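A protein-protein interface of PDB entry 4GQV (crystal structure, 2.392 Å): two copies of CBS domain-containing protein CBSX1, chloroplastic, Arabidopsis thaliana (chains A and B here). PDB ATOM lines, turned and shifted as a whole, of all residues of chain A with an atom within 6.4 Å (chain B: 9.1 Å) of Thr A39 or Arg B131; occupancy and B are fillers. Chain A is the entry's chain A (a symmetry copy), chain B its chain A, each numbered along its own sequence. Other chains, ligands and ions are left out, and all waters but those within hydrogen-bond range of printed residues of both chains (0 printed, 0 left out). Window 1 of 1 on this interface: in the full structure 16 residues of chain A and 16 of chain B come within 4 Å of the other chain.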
ATOM      1  N   LEU A  33      10.801 -28.360   8.787  1.00  0.00           N
ATOM      2  CA  LEU A  33       9.882 -27.795   7.810  1.00  0.00           C
ATOM      3  C   LEU A  33       9.931 -26.287   7.836  1.00  0.00           C
ATOM      4  O   LEU A  33       9.953 -25.651   6.781  1.00  0.00           O
ATOM      5  CB  LEU A  33       8.444 -28.232   8.077  1.00  0.00           C
ATOM      6  CG  LEU A  33       8.014 -29.671   7.815  1.00  0.00           C
ATOM      7  CD1 LEU A  33       6.552 -29.859   8.176  1.00  0.00           C
ATOM      8  CD2 LEU A  33       8.261 -30.055   6.363  1.00  0.00           C
ATOM      9  N   ARG A  37      11.491 -24.550   4.538  1.00  0.00           N
ATOM     10  CA  ARG A  37      10.333 -24.221   3.710  1.00  0.00           C
ATOM     11  C   ARG A  37       9.796 -25.401   2.889  1.00  0.00           C
ATOM     12  O   ARG A  37       9.443 -25.249   1.718  1.00  0.00           O
ATOM     13  CB  ARG A  37      10.632 -23.023   2.803  1.00  0.00           C
ATOM     14  CG  ARG A  37       9.424 -22.130   2.583  1.00  0.00           C
ATOM     15  CD  ARG A  37       9.595 -21.227   1.373  1.00  0.00           C
ATOM     16  NE  ARG A  37       8.355 -20.528   1.048  1.00  0.00           N
ATOM     17  CZ  ARG A  37       8.086 -19.990  -0.138  1.00  0.00           C
ATOM     18  NH1 ARG A  37       8.970 -20.076  -1.122  1.00  0.00           N
ATOM     19  NH2 ARG A  37       6.928 -19.372  -0.345  1.00  0.00           N
ATOM     20  N   ILE A  38       9.740 -26.574   3.508  1.00  0.00           N
ATOM     21  CA  ILE A  38       9.159 -27.749   2.869  1.00  0.00           C
ATOM     22  C   ILE A  38       7.822 -28.130   3.503  1.00  0.00           C
ATOM     23  O   ILE A  38       7.481 -27.657   4.587  1.00  0.00           O
ATOM     24  CB  ILE A  38      10.121 -28.947   2.909  1.00  0.00           C
ATOM     25  CG1 ILE A  38      11.240 -28.701   3.924  1.00  0.00           C
ATOM     26  CG2 ILE A  38      10.715 -29.180   1.535  1.00  0.00           C
ATOM     27  CD1 ILE A  38      12.385 -29.675   3.800  1.00  0.00           C
ATOM     28  N   THR A  39       7.057 -28.974   2.823  1.00  0.00           N
ATOM     29  CA  THR A  39       5.783 -29.428   3.387  1.00  0.00           C
ATOM     30  C   THR A  39       5.812 -30.923   3.664  1.00  0.00           C
ATOM     31  O   THR A  39       4.774 -31.566   3.790  1.00  0.00           O
ATOM     32  CB  THR A  39       4.593 -29.088   2.480  1.00  0.00           C
ATOM     33  OG1 THR A  39       4.743 -29.764   1.228  1.00  0.00           O
ATOM     34  CG2 THR A  39       4.518 -27.582   2.244  1.00  0.00           C
ATOM     35  N   GLY A  40       7.016 -31.470   3.762  1.00  0.00           N
ATOM     36  CA  GLY A  40       7.173 -32.890   4.001  1.00  0.00           C
ATOM     37  C   GLY A  40       8.593 -33.348   3.748  1.00  0.00           C
ATOM     38  O   GLY A  40       9.411 -32.589   3.239  1.00  0.00           O
ATOM     39  N   PHE A  41       8.891 -34.582   4.127  1.00  0.00           N
ATOM     40  CA  PHE A  41      10.197 -35.165   3.871  1.00  0.00           C
ATOM     41  C   PHE A  41       9.987 -36.632   3.586  1.00  0.00           C
ATOM     42  O   PHE A  41       8.985 -37.216   4.026  1.00  0.00           O
ATOM     43  CB  PHE A  41      11.137 -35.125   5.105  1.00  0.00           C
ATOM     44  CG  PHE A  41      10.857 -34.026   6.094  1.00  0.00           C
ATOM     45  CD1 PHE A  41      11.753 -32.985   6.240  1.00  0.00           C
ATOM     46  CD2 PHE A  41       9.738 -34.060   6.908  1.00  0.00           C
ATOM     47  CE1 PHE A  41      11.525 -31.970   7.158  1.00  0.00           C
ATOM     48  CE2 PHE A  41       9.500 -33.035   7.825  1.00  0.00           C
ATOM     49  CZ  PHE A  41      10.407 -32.005   7.952  1.00  0.00           C
ATOM     50  N   VAL A  54       6.474 -38.243   5.011  1.00  0.00           N
ATOM     51  CA  VAL A  54       5.733 -37.562   6.046  1.00  0.00           C
ATOM     52  C   VAL A  54       5.499 -36.119   5.667  1.00  0.00           C
ATOM     53  O   VAL A  54       6.341 -35.495   5.040  1.00  0.00           O
ATOM     54  CB  VAL A  54       6.407 -37.692   7.433  1.00  0.00           C
ATOM     55  CG1 VAL A  54       7.504 -36.656   7.618  1.00  0.00           C
ATOM     56  CG2 VAL A  54       5.357 -37.564   8.522  1.00  0.00           C
ATOM     57  N   SER A  55       4.313 -35.610   6.004  1.00  0.00           N
ATOM     58  CA  SER A  55       3.941 -34.249   5.604  1.00  0.00           C
ATOM     59  C   SER A  55       3.381 -33.439   6.786  1.00  0.00           C
ATOM     60  O   SER A  55       3.013 -34.001   7.819  1.00  0.00           O
ATOM     61  CB  SER A  55       2.911 -34.298   4.475  1.00  0.00           C
ATOM     62  OG  SER A  55       1.765 -35.007   4.911  1.00  0.00           O
ATOM     63  N   ASP A  56       3.297 -32.124   6.602  1.00  0.00           N
ATOM     64  CA  ASP A  56       2.723 -31.234   7.610  1.00  0.00           C
ATOM     65  C   ASP A  56       1.328 -31.682   8.090  1.00  0.00           C
ATOM     66  O   ASP A  56       1.053 -31.688   9.282  1.00  0.00           O
ATOM     67  CB  ASP A  56       2.705 -29.794   7.109  1.00  0.00           C
ATOM     68  CG  ASP A  56       1.854 -29.609   5.853  1.00  0.00           C
ATOM     69  OD1 ASP A  56       1.185 -30.573   5.395  1.00  0.00           O
ATOM     70  OD2 ASP A  56       1.841 -28.469   5.334  1.00  0.00           O
ATOM     71  N   TYR A  57       0.477 -32.097   7.157  1.00  0.00           N
ATOM     72  CA  TYR A  57      -0.836 -32.664   7.481  1.00  0.00           C
ATOM     73  C   TYR A  57      -0.734 -33.845   8.449  1.00  0.00           C
ATOM     74  O   TYR A  57      -1.564 -33.998   9.352  1.00  0.00           O
ATOM     75  CB  TYR A  57      -1.565 -33.081   6.195  1.00  0.00           C
ATOM     76  CG  TYR A  57      -2.865 -33.843   6.398  1.00  0.00           C
ATOM     77  CD1 TYR A  57      -4.087 -33.175   6.455  1.00  0.00           C
ATOM     78  CD2 TYR A  57      -2.877 -35.234   6.501  1.00  0.00           C
ATOM     79  CE1 TYR A  57      -5.283 -33.873   6.629  1.00  0.00           C
ATOM     80  CE2 TYR A  57      -4.068 -35.939   6.683  1.00  0.00           C
ATOM     81  CZ  TYR A  57      -5.264 -35.255   6.742  1.00  0.00           C
ATOM     82  OH  TYR A  57      -6.443 -35.950   6.917  1.00  0.00           O
ATOM     83  N   ARG A 131       3.313 -34.502  -6.024  1.00  0.00           N
ATOM     84  CA  ARG A 131       4.191 -33.409  -6.420  1.00  0.00           C
ATOM     85  C   ARG A 131       5.642 -33.830  -6.262  1.00  0.00           C
ATOM     86  O   ARG A 131       6.541 -33.183  -6.772  1.00  0.00           O
ATOM     87  CB  ARG A 131       3.928 -32.180  -5.551  1.00  0.00           C
ATOM     88  CG  ARG A 131       2.807 -31.298  -6.015  1.00  0.00           C
ATOM     89  CD  ARG A 131       3.260 -29.861  -5.962  1.00  0.00           C
ATOM     90  NE  ARG A 131       2.283 -28.963  -6.564  1.00  0.00           N
ATOM     91  CZ  ARG A 131       1.330 -28.333  -5.886  1.00  0.00           C
ATOM     92  NH1 ARG A 131       1.223 -28.497  -4.574  1.00  0.00           N
ATOM     93  NH2 ARG A 131       0.487 -27.533  -6.516  1.00  0.00           N
ATOM     94  N   ARG A 132       5.849 -34.916  -5.536  1.00  0.00           N
ATOM     95  CA  ARG A 132       7.173 -35.434  -5.237  1.00  0.00           C
ATOM     96  C   ARG A 132       7.134 -36.931  -5.521  1.00  0.00           C
ATOM     97  O   ARG A 132       6.055 -37.512  -5.539  1.00  0.00           O
ATOM     98  CB  ARG A 132       7.533 -35.152  -3.756  1.00  0.00           C
ATOM     99  CG  ARG A 132       7.307 -33.670  -3.360  1.00  0.00           C
ATOM    100  CD  ARG A 132       7.657 -33.358  -1.905  1.00  0.00           C
ATOM    101  NE  ARG A 132       6.548 -32.747  -1.159  1.00  0.00           N
ATOM    102  CZ  ARG A 132       6.377 -32.876   0.156  1.00  0.00           C
ATOM    103  NH1 ARG A 132       7.222 -33.604   0.864  1.00  0.00           N
ATOM    104  NH2 ARG A 132       5.351 -32.296   0.763  1.00  0.00           N
ATOM    105  N   THR B  12       4.169 -13.841   5.790  1.00  0.00           N
ATOM    106  CA  THR B  12       5.181 -13.542   4.815  1.00  0.00           C
ATOM    107  C   THR B  12       4.918 -12.123   4.281  1.00  0.00           C
ATOM    108  O   THR B  12       3.972 -11.886   3.514  1.00  0.00           O
ATOM    109  CB  THR B  12       5.150 -14.598   3.690  1.00  0.00           C
ATOM    110  OG1 THR B  12       5.353 -15.904   4.261  1.00  0.00           O
ATOM    111  CG2 THR B  12       6.227 -14.315   2.638  1.00  0.00           C
ATOM    112  N   ARG B  37      11.213 -21.947  -5.980  1.00  0.00           N
ATOM    113  CA  ARG B  37      10.718 -23.157  -5.326  1.00  0.00           C
ATOM    114  C   ARG B  37       9.321 -23.006  -4.709  1.00  0.00           C
ATOM    115  O   ARG B  37       9.062 -23.483  -3.603  1.00  0.00           O
ATOM    116  CB  ARG B  37      11.718 -23.663  -4.283  1.00  0.00           C
ATOM    117  CG  ARG B  37      11.759 -25.178  -4.185  1.00  0.00           C
ATOM    118  CD  ARG B  37      12.398 -25.649  -2.891  1.00  0.00           C
ATOM    119  NE  ARG B  37      12.245 -27.091  -2.712  1.00  0.00           N
ATOM    120  CZ  ARG B  37      12.348 -27.717  -1.543  1.00  0.00           C
ATOM    121  NH1 ARG B  37      12.598 -27.027  -0.439  1.00  0.00           N
ATOM    122  NH2 ARG B  37      12.191 -29.034  -1.475  1.00  0.00           N
ATOM    123  N   THR B  39       4.878 -23.257  -5.399  1.00  0.00           N
ATOM    124  CA  THR B  39       3.904 -24.000  -6.199  1.00  0.00           C
ATOM    125  C   THR B  39       2.734 -23.112  -6.596  1.00  0.00           C
ATOM    126  O   THR B  39       1.659 -23.594  -6.945  1.00  0.00           O
ATOM    127  CB  THR B  39       3.387 -25.249  -5.472  1.00  0.00           C
ATOM    128  OG1 THR B  39       2.708 -24.854  -4.276  1.00  0.00           O
ATOM    129  CG2 THR B  39       4.545 -26.178  -5.122  1.00  0.00           C
ATOM    130  N   LEU B  53      -5.238 -15.968  -7.732  1.00  0.00           N
ATOM    131  CA  LEU B  53      -4.218 -16.879  -7.253  1.00  0.00           C
ATOM    132  C   LEU B  53      -3.937 -17.845  -8.381  1.00  0.00           C
ATOM    133  O   LEU B  53      -4.830 -18.140  -9.193  1.00  0.00           O
ATOM    134  CB  LEU B  53      -4.717 -17.660  -6.043  1.00  0.00           C
ATOM    135  CG  LEU B  53      -4.660 -16.921  -4.708  1.00  0.00           C
ATOM    136  CD1 LEU B  53      -5.147 -17.817  -3.588  1.00  0.00           C
ATOM    137  CD2 LEU B  53      -3.238 -16.487  -4.438  1.00  0.00           C
ATOM    138  N   ALA B 121      -7.127 -17.397  11.217  1.00  0.00           N
ATOM    139  CA  ALA B 121      -6.283 -17.823  10.111  1.00  0.00           C
ATOM    140  C   ALA B 121      -5.812 -19.235  10.352  1.00  0.00           C
ATOM    141  O   ALA B 121      -5.846 -20.062   9.466  1.00  0.00           O
ATOM    142  CB  ALA B 121      -5.097 -16.899   9.979  1.00  0.00           C
ATOM    143  N   ILE B 124      -8.482 -21.822   9.714  1.00  0.00           N
ATOM    144  CA  ILE B 124      -8.658 -22.118   8.294  1.00  0.00           C
ATOM    145  C   ILE B 124      -7.519 -22.979   7.767  1.00  0.00           C
ATOM    146  O   ILE B 124      -7.737 -24.057   7.216  1.00  0.00           O
ATOM    147  CB  ILE B 124      -8.747 -20.855   7.431  1.00  0.00           C
ATOM    148  CG1 ILE B 124      -9.941 -20.002   7.861  1.00  0.00           C
ATOM    149  CG2 ILE B 124      -8.862 -21.251   5.974  1.00  0.00           C
ATOM    150  CD1 ILE B 124     -11.225 -20.770   7.864  1.00  0.00           C
ATOM    151  N   LEU B 125      -6.300 -22.498   7.949  1.00  0.00           N
ATOM    152  CA  LEU B 125      -5.134 -23.227   7.496  1.00  0.00           C
ATOM    153  C   LEU B 125      -5.148 -24.675   7.974  1.00  0.00           C
ATOM    154  O   LEU B 125      -4.819 -25.585   7.221  1.00  0.00           O
ATOM    155  CB  LEU B 125      -3.854 -22.535   7.960  1.00  0.00           C
ATOM    156  CG  LEU B 125      -3.263 -21.439   7.063  1.00  0.00           C
ATOM    157  CD1 LEU B 125      -3.726 -21.582   5.601  1.00  0.00           C
ATOM    158  CD2 LEU B 125      -3.547 -20.044   7.599  1.00  0.00           C
ATOM    159  N   LEU B 126      -5.566 -24.887   9.214  1.00  0.00           N
ATOM    160  CA  LEU B 126      -5.437 -26.200   9.831  1.00  0.00           C
ATOM    161  C   LEU B 126      -6.644 -27.116   9.639  1.00  0.00           C
ATOM    162  O   LEU B 126      -6.607 -28.262  10.045  1.00  0.00           O
ATOM    163  CB  LEU B 126      -5.094 -26.061  11.321  1.00  0.00           C
ATOM    164  CG  LEU B 126      -3.786 -25.334  11.663  1.00  0.00           C
ATOM    165  CD1 LEU B 126      -3.761 -24.917  13.131  1.00  0.00           C
ATOM    166  CD2 LEU B 126      -2.573 -26.184  11.310  1.00  0.00           C
ATOM    167  N   GLU B 127      -7.709 -26.619   9.024  1.00  0.00           N
ATOM    168  CA  GLU B 127      -8.916 -27.422   8.843  1.00  0.00           C
ATOM    169  C   GLU B 127      -9.345 -27.534   7.378  1.00  0.00           C
ATOM    170  O   GLU B 127     -10.448 -27.991   7.082  1.00  0.00           O
ATOM    171  CB  GLU B 127     -10.075 -26.818   9.639  1.00  0.00           C
ATOM    172  CG  GLU B 127     -10.106 -27.139  11.119  1.00  0.00           C
ATOM    173  CD  GLU B 127     -11.265 -26.434  11.814  1.00  0.00           C
ATOM    174  OE1 GLU B 127     -11.624 -26.819  12.956  1.00  0.00           O
ATOM    175  OE2 GLU B 127     -11.813 -25.489  11.199  1.00  0.00           O
ATOM    176  N   THR B 128      -8.484 -27.103   6.465  1.00  0.00           N
ATOM    177  CA  THR B 128      -8.836 -27.036   5.051  1.00  0.00           C
ATOM    178  C   THR B 128      -7.653 -27.342   4.146  1.00  0.00           C
ATOM    179  O   THR B 128      -6.499 -27.368   4.577  1.00  0.00           O
ATOM    180  CB  THR B 128      -9.320 -25.622   4.652  1.00  0.00           C
ATOM    181  OG1 THR B 128      -8.230 -24.696   4.767  1.00  0.00           O
ATOM    182  CG2 THR B 128     -10.497 -25.150   5.513  1.00  0.00           C
ATOM    183  N   LYS B 129      -7.957 -27.537   2.869  1.00  0.00           N
ATOM    184  CA  LYS B 129      -6.951 -27.798   1.846  1.00  0.00           C
ATOM    185  C   LYS B 129      -5.972 -26.634   1.676  1.00  0.00           C
ATOM    186  O   LYS B 129      -4.909 -26.781   1.059  1.00  0.00           O
ATOM    187  CB  LYS B 129      -7.649 -28.096   0.513  1.00  0.00           C
ATOM    188  CG  LYS B 129      -8.531 -29.347   0.527  1.00  0.00           C
ATOM    189  CD  LYS B 129     -10.010 -29.035   0.265  1.00  0.00           C
ATOM    190  CE  LYS B 129     -10.869 -30.295   0.437  1.00  0.00           C
ATOM    191  NZ  LYS B 129     -12.329 -30.040   0.305  1.00  0.00           N
ATOM    192  N   TYR B 130      -6.337 -25.480   2.222  1.00  0.00           N
ATOM    193  CA  TYR B 130      -5.552 -24.254   2.063  1.00  0.00           C
ATOM    194  C   TYR B 130      -4.256 -24.239   2.897  1.00  0.00           C
ATOM    195  O   TYR B 130      -4.263 -24.454   4.116  1.00  0.00           O
ATOM    196  CB  TYR B 130      -6.418 -23.022   2.377  1.00  0.00           C
ATOM    197  CG  TYR B 130      -7.725 -22.966   1.602  1.00  0.00           C
ATOM    198  CD1 TYR B 130      -7.752 -22.594   0.264  1.00  0.00           C
ATOM    199  CD2 TYR B 130      -8.931 -23.281   2.216  1.00  0.00           C
ATOM    200  CE1 TYR B 130      -8.946 -22.543  -0.445  1.00  0.00           C
ATOM    201  CE2 TYR B 130     -10.131 -23.240   1.529  1.00  0.00           C
ATOM    202  CZ  TYR B 130     -10.134 -22.871   0.195  1.00  0.00           C
ATOM    203  OH  TYR B 130     -11.334 -22.830  -0.475  1.00  0.00           O
ATOM    204  N   ARG B 131      -3.148 -23.995   2.210  1.00  0.00           N
ATOM    205  CA  ARG B 131      -1.835 -23.922   2.836  1.00  0.00           C
ATOM    206  C   ARG B 131      -1.364 -22.478   2.881  1.00  0.00           C
ATOM    207  O   ARG B 131      -0.424 -22.146   3.584  1.00  0.00           O
ATOM    208  CB  ARG B 131      -0.826 -24.752   2.045  1.00  0.00           C
ATOM    209  CG  ARG B 131      -0.786 -26.210   2.395  1.00  0.00           C
ATOM    210  CD  ARG B 131       0.651 -26.642   2.541  1.00  0.00           C
ATOM    211  NE  ARG B 131       0.759 -28.002   3.052  1.00  0.00           N
ATOM    212  CZ  ARG B 131       0.869 -29.081   2.285  1.00  0.00           C
ATOM    213  NH1 ARG B 131       0.889 -28.964   0.965  1.00  0.00           N
ATOM    214  NH2 ARG B 131       0.964 -30.280   2.837  1.00  0.00           N
ATOM    215  N   ARG B 132      -2.027 -21.634   2.106  1.00  0.00           N
ATOM    216  CA  ARG B 132      -1.683 -20.228   1.983  1.00  0.00           C
ATOM    217  C   ARG B 132      -2.981 -19.443   2.126  1.00  0.00           C
ATOM    218  O   ARG B 132      -4.050 -20.006   1.918  1.00  0.00           O
ATOM    219  CB  ARG B 132      -1.013 -19.962   0.610  1.00  0.00           C
ATOM    220  CG  ARG B 132       0.146 -20.947   0.312  1.00  0.00           C
ATOM    221  CD  ARG B 132       0.831 -20.707  -1.034  1.00  0.00           C
ATOM    222  NE  ARG B 132       0.851 -21.899  -1.894  1.00  0.00           N
ATOM    223  CZ  ARG B 132       0.865 -21.853  -3.226  1.00  0.00           C
ATOM    224  NH1 ARG B 132       0.843 -20.688  -3.848  1.00  0.00           N
ATOM    225  NH2 ARG B 132       0.882 -22.971  -3.939  1.00  0.00           N
ATOM    226  N   LEU B 133      -2.885 -18.175   2.526  1.00  0.00           N
ATOM    227  CA  LEU B 133      -3.991 -17.220   2.451  1.00  0.00           C
ATOM    228  C   LEU B 133      -3.396 -15.855   2.199  1.00  0.00           C
ATOM    229  O   LEU B 133      -2.507 -15.436   2.905  1.00  0.00           O
ATOM    230  CB  LEU B 133      -4.812 -17.162   3.733  1.00  0.00           C
ATOM    231  CG  LEU B 133      -5.651 -18.391   4.114  1.00  0.00           C
ATOM    232  CD1 LEU B 133      -6.348 -18.165   5.464  1.00  0.00           C
ATOM    233  CD2 LEU B 133      -6.659 -18.751   3.027  1.00  0.00           C
ATOM    234  N   PRO B 134      -3.886 -15.155   1.173  1.00  0.00           N
ATOM    235  CA  PRO B 134      -3.378 -13.805   0.950  1.00  0.00           C
ATOM    236  C   PRO B 134      -3.865 -12.842   2.036  1.00  0.00           C
ATOM    237  O   PRO B 134      -4.983 -12.964   2.541  1.00  0.00           O
ATOM    238  CB  PRO B 134      -3.950 -13.431  -0.422  1.00  0.00           C
ATOM    239  CG  PRO B 134      -5.096 -14.359  -0.649  1.00  0.00           C
ATOM    240  CD  PRO B 134      -4.817 -15.605   0.126  1.00  0.00           C
ATOM    241  N   ILE B 145       1.145 -12.713   2.748  1.00  0.00           N
ATOM    242  CA  ILE B 145       0.510 -14.020   2.700  1.00  0.00           C
ATOM    243  C   ILE B 145       0.819 -14.751   4.018  1.00  0.00           C
ATOM    244  O   ILE B 145       1.915 -14.625   4.569  1.00  0.00           O
ATOM    245  CB  ILE B 145       1.009 -14.849   1.475  1.00  0.00           C
ATOM    246  CG1 ILE B 145       0.371 -14.337   0.182  1.00  0.00           C
ATOM    247  CG2 ILE B 145       0.688 -16.297   1.635  1.00  0.00           C
ATOM    248  CD1 ILE B 145       0.567 -15.237  -1.007  1.00  0.00           C
ATOM    249  N   ILE B 146      -0.165 -15.478   4.542  1.00  0.00           N
ATOM    250  CA  ILE B 146       0.056 -16.357   5.666  1.00  0.00           C
ATOM    251  C   ILE B 146      -0.102 -17.826   5.277  1.00  0.00           C
ATOM    252  O   ILE B 146      -1.160 -18.286   4.840  1.00  0.00           O
ATOM    253  CB  ILE B 146      -0.877 -16.035   6.842  1.00  0.00           C
ATOM    254  CG1 ILE B 146      -0.704 -17.082   7.936  1.00  0.00           C
ATOM    255  CG2 ILE B 146      -2.339 -15.931   6.383  1.00  0.00           C
ATOM    256  CD1 ILE B 146       0.286 -16.687   8.987  1.00  0.00           C
ATOM    257  N   THR B 147       0.980 -18.564   5.447  1.00  0.00           N
ATOM    258  CA  THR B 147       0.972 -19.982   5.153  1.00  0.00           C
ATOM    259  C   THR B 147       0.846 -20.789   6.447  1.00  0.00           C
ATOM    260  O   THR B 147       1.092 -20.273   7.533  1.00  0.00           O
ATOM    261  CB  THR B 147       2.235 -20.380   4.389  1.00  0.00           C
ATOM    262  OG1 THR B 147       3.178 -20.932   5.305  1.00  0.00           O
ATOM    263  CG2 THR B 147       2.838 -19.167   3.742  1.00  0.00           C
ATOM    264  N   ARG B 148       0.433 -22.046   6.315  1.00  0.00           N
ATOM    265  CA  ARG B 148       0.361 -23.000   7.420  1.00  0.00           C
ATOM    266  C   ARG B 148       1.743 -23.139   8.075  1.00  0.00           C
ATOM    267  O   ARG B 148       1.852 -23.356   9.288  1.00  0.00           O
ATOM    268  CB  ARG B 148      -0.134 -24.360   6.883  1.00  0.00           C
ATOM    269  CG  ARG B 148      -0.414 -25.452   7.916  1.00  0.00           C
ATOM    270  CD  ARG B 148      -0.828 -26.772   7.246  1.00  0.00           C
ATOM    271  NE  ARG B 148      -2.193 -26.714   6.720  1.00  0.00           N
ATOM    272  CZ  ARG B 148      -2.711 -27.589   5.861  1.00  0.00           C
ATOM    273  NH1 ARG B 148      -1.977 -28.612   5.417  1.00  0.00           N
ATOM    274  NH2 ARG B 148      -3.958 -27.437   5.438  1.00  0.00           N
ATOM    275  N   GLY B 149       2.788 -23.021   7.252  1.00  0.00           N
ATOM    276  CA  GLY B 149       4.147 -22.944   7.736  1.00  0.00           C
ATOM    277  C   GLY B 149       4.305 -21.804   8.734  1.00  0.00           C
ATOM    278  O   GLY B 149       4.697 -22.024   9.870  1.00  0.00           O
ATOM    279  N   ASN B 150       4.007 -20.587   8.297  1.00  0.00           N
ATOM    280  CA  ASN B 150       4.078 -19.413   9.151  1.00  0.00           C
ATOM    281  C   ASN B 150       3.325 -19.616  10.470  1.00  0.00           C
ATOM    282  O   ASN B 150       3.808 -19.235  11.545  1.00  0.00           O
ATOM    283  CB  ASN B 150       3.523 -18.200   8.399  1.00  0.00           C
ATOM    284  CG  ASN B 150       4.395 -17.799   7.225  1.00  0.00           C
ATOM    285  OD1 ASN B 150       5.580 -18.100   7.200  1.00  0.00           O
ATOM    286  ND2 ASN B 150       3.816 -17.098   6.255  1.00  0.00           N
ATOM    287  N   VAL B 151       2.155 -20.246  10.392  1.00  0.00           N
ATOM    288  CA  VAL B 151       1.386 -20.555  11.595  1.00  0.00           C
ATOM    289  C   VAL B 151       2.159 -21.511  12.496  1.00  0.00           C
ATOM    290  O   VAL B 151       2.198 -21.327  13.720  1.00  0.00           O
ATOM    291  CB  VAL B 151       0.005 -21.160  11.269  1.00  0.00           C
ATOM    292  CG1 VAL B 151      -0.651 -21.712  12.534  1.00  0.00           C
ATOM    293  CG2 VAL B 151      -0.898 -20.117  10.601  1.00  0.00           C
ATOM    294  N   VAL B 152       2.770 -22.529  11.887  1.00  0.00           N
ATOM    295  CA  VAL B 152       3.575 -23.509  12.622  1.00  0.00           C
ATOM    296  C   VAL B 152       4.733 -22.826  13.349  1.00  0.00           C
ATOM    297  O   VAL B 152       4.929 -23.032  14.544  1.00  0.00           O
ATOM    298  CB  VAL B 152       4.110 -24.632  11.689  1.00  0.00           C
ATOM    299  CG1 VAL B 152       5.304 -25.312  12.312  1.00  0.00           C
ATOM    300  CG2 VAL B 152       3.022 -25.652  11.396  1.00  0.00           C
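Of chain B, only Arg B131 (3.7 Å) comes within 4 Å of Thr A39. Arg B131 touches just these residues of chain A: Thr A39 and Asp A56. No residue of chain B comes within 4 Å of Gly A40. No residue of chain B comes within 4 Å of Ser A55. Of the printed residues of chain A, Thr B39 touches Arg A131 (3.7 Å). Printed residues of chain B within 4 Å of Arg A131: Thr B39 (3.7 Å). Of the printed residues of chain A, Arg B37 touches Ile A38 (3.4 Å). Of the printed residues of chain A, Arg B148 touches Asp A56 (3.7 Å). The nearest residue of chain B that does not touch Thr A39 is Arg B37 (6.7 Å). The nearest residue of chain A that does not touch Arg B131 is Tyr A57 (4.7 Å).
NE of Arg B131 is in salt-bridge range of OD2 of Asp A56, 2.6 Å away. The side-chain carboxylate (OD1) of Asp A56 lies within salt-bridge range of the guanidinium group (NH1) of Arg B148 (3.7 Å).
CG2 of Ile A38 touches NH2 of Arg B37, at 3.4 Å. Arg B131 touches Thr A39. Arg A131 touches Thr B39.
Thr A39 touches Arg B131, and with the chains exchanged Arg A131 touches Thr B39. Of the 5 pairs that touch across the chains among the printed residues, 2 have their exchanged pair printed and touching as well.
The backbone carbonyl oxygen (O) of Thr B128 lies within hydrogen-bond range of the guanidinium group (NH2) of Arg B148. N of Asp A56 is in hydrogen-bond range of O of Thr A39 (3.2 Å). NH2 of Arg A132 sits at hydrogen-bond distance from OG1 of Thr A39 (2.6 Å). NH2 of Arg B148 is in hydrogen-bond range of O of Tyr B130 (3.3 Å). The backbone carbonyl oxygen of Arg B131 is in hydrogen-bond range of the backbone NH of Arg B148, at 2.9 Å. The backbone carbonyl oxygen (O) of Leu A33 is in hydrogen-bond range of the backbone NH (N) of Ile A38, 3.4 Å away.
Of the 24 printed residues of chain B, 4 touch a printed residue of chain A. Printed residues of chain B that touch a printed residue of chain A: Arg B37, Thr B39, Arg B131 and Arg B148. Of the 12 printed residues of chain A, 4 touch a printed residue of chain B. Among the printed residues, 5 pairs touch across the chains. Among the printed residues, Asp or Glu carboxylates within 4 Å of a Lys or Arg side-chain nitrogen of the other chain: Asp A56 with Arg B131 (2.6 Å) and Asp A56 with Arg B148 (3.7 Å).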
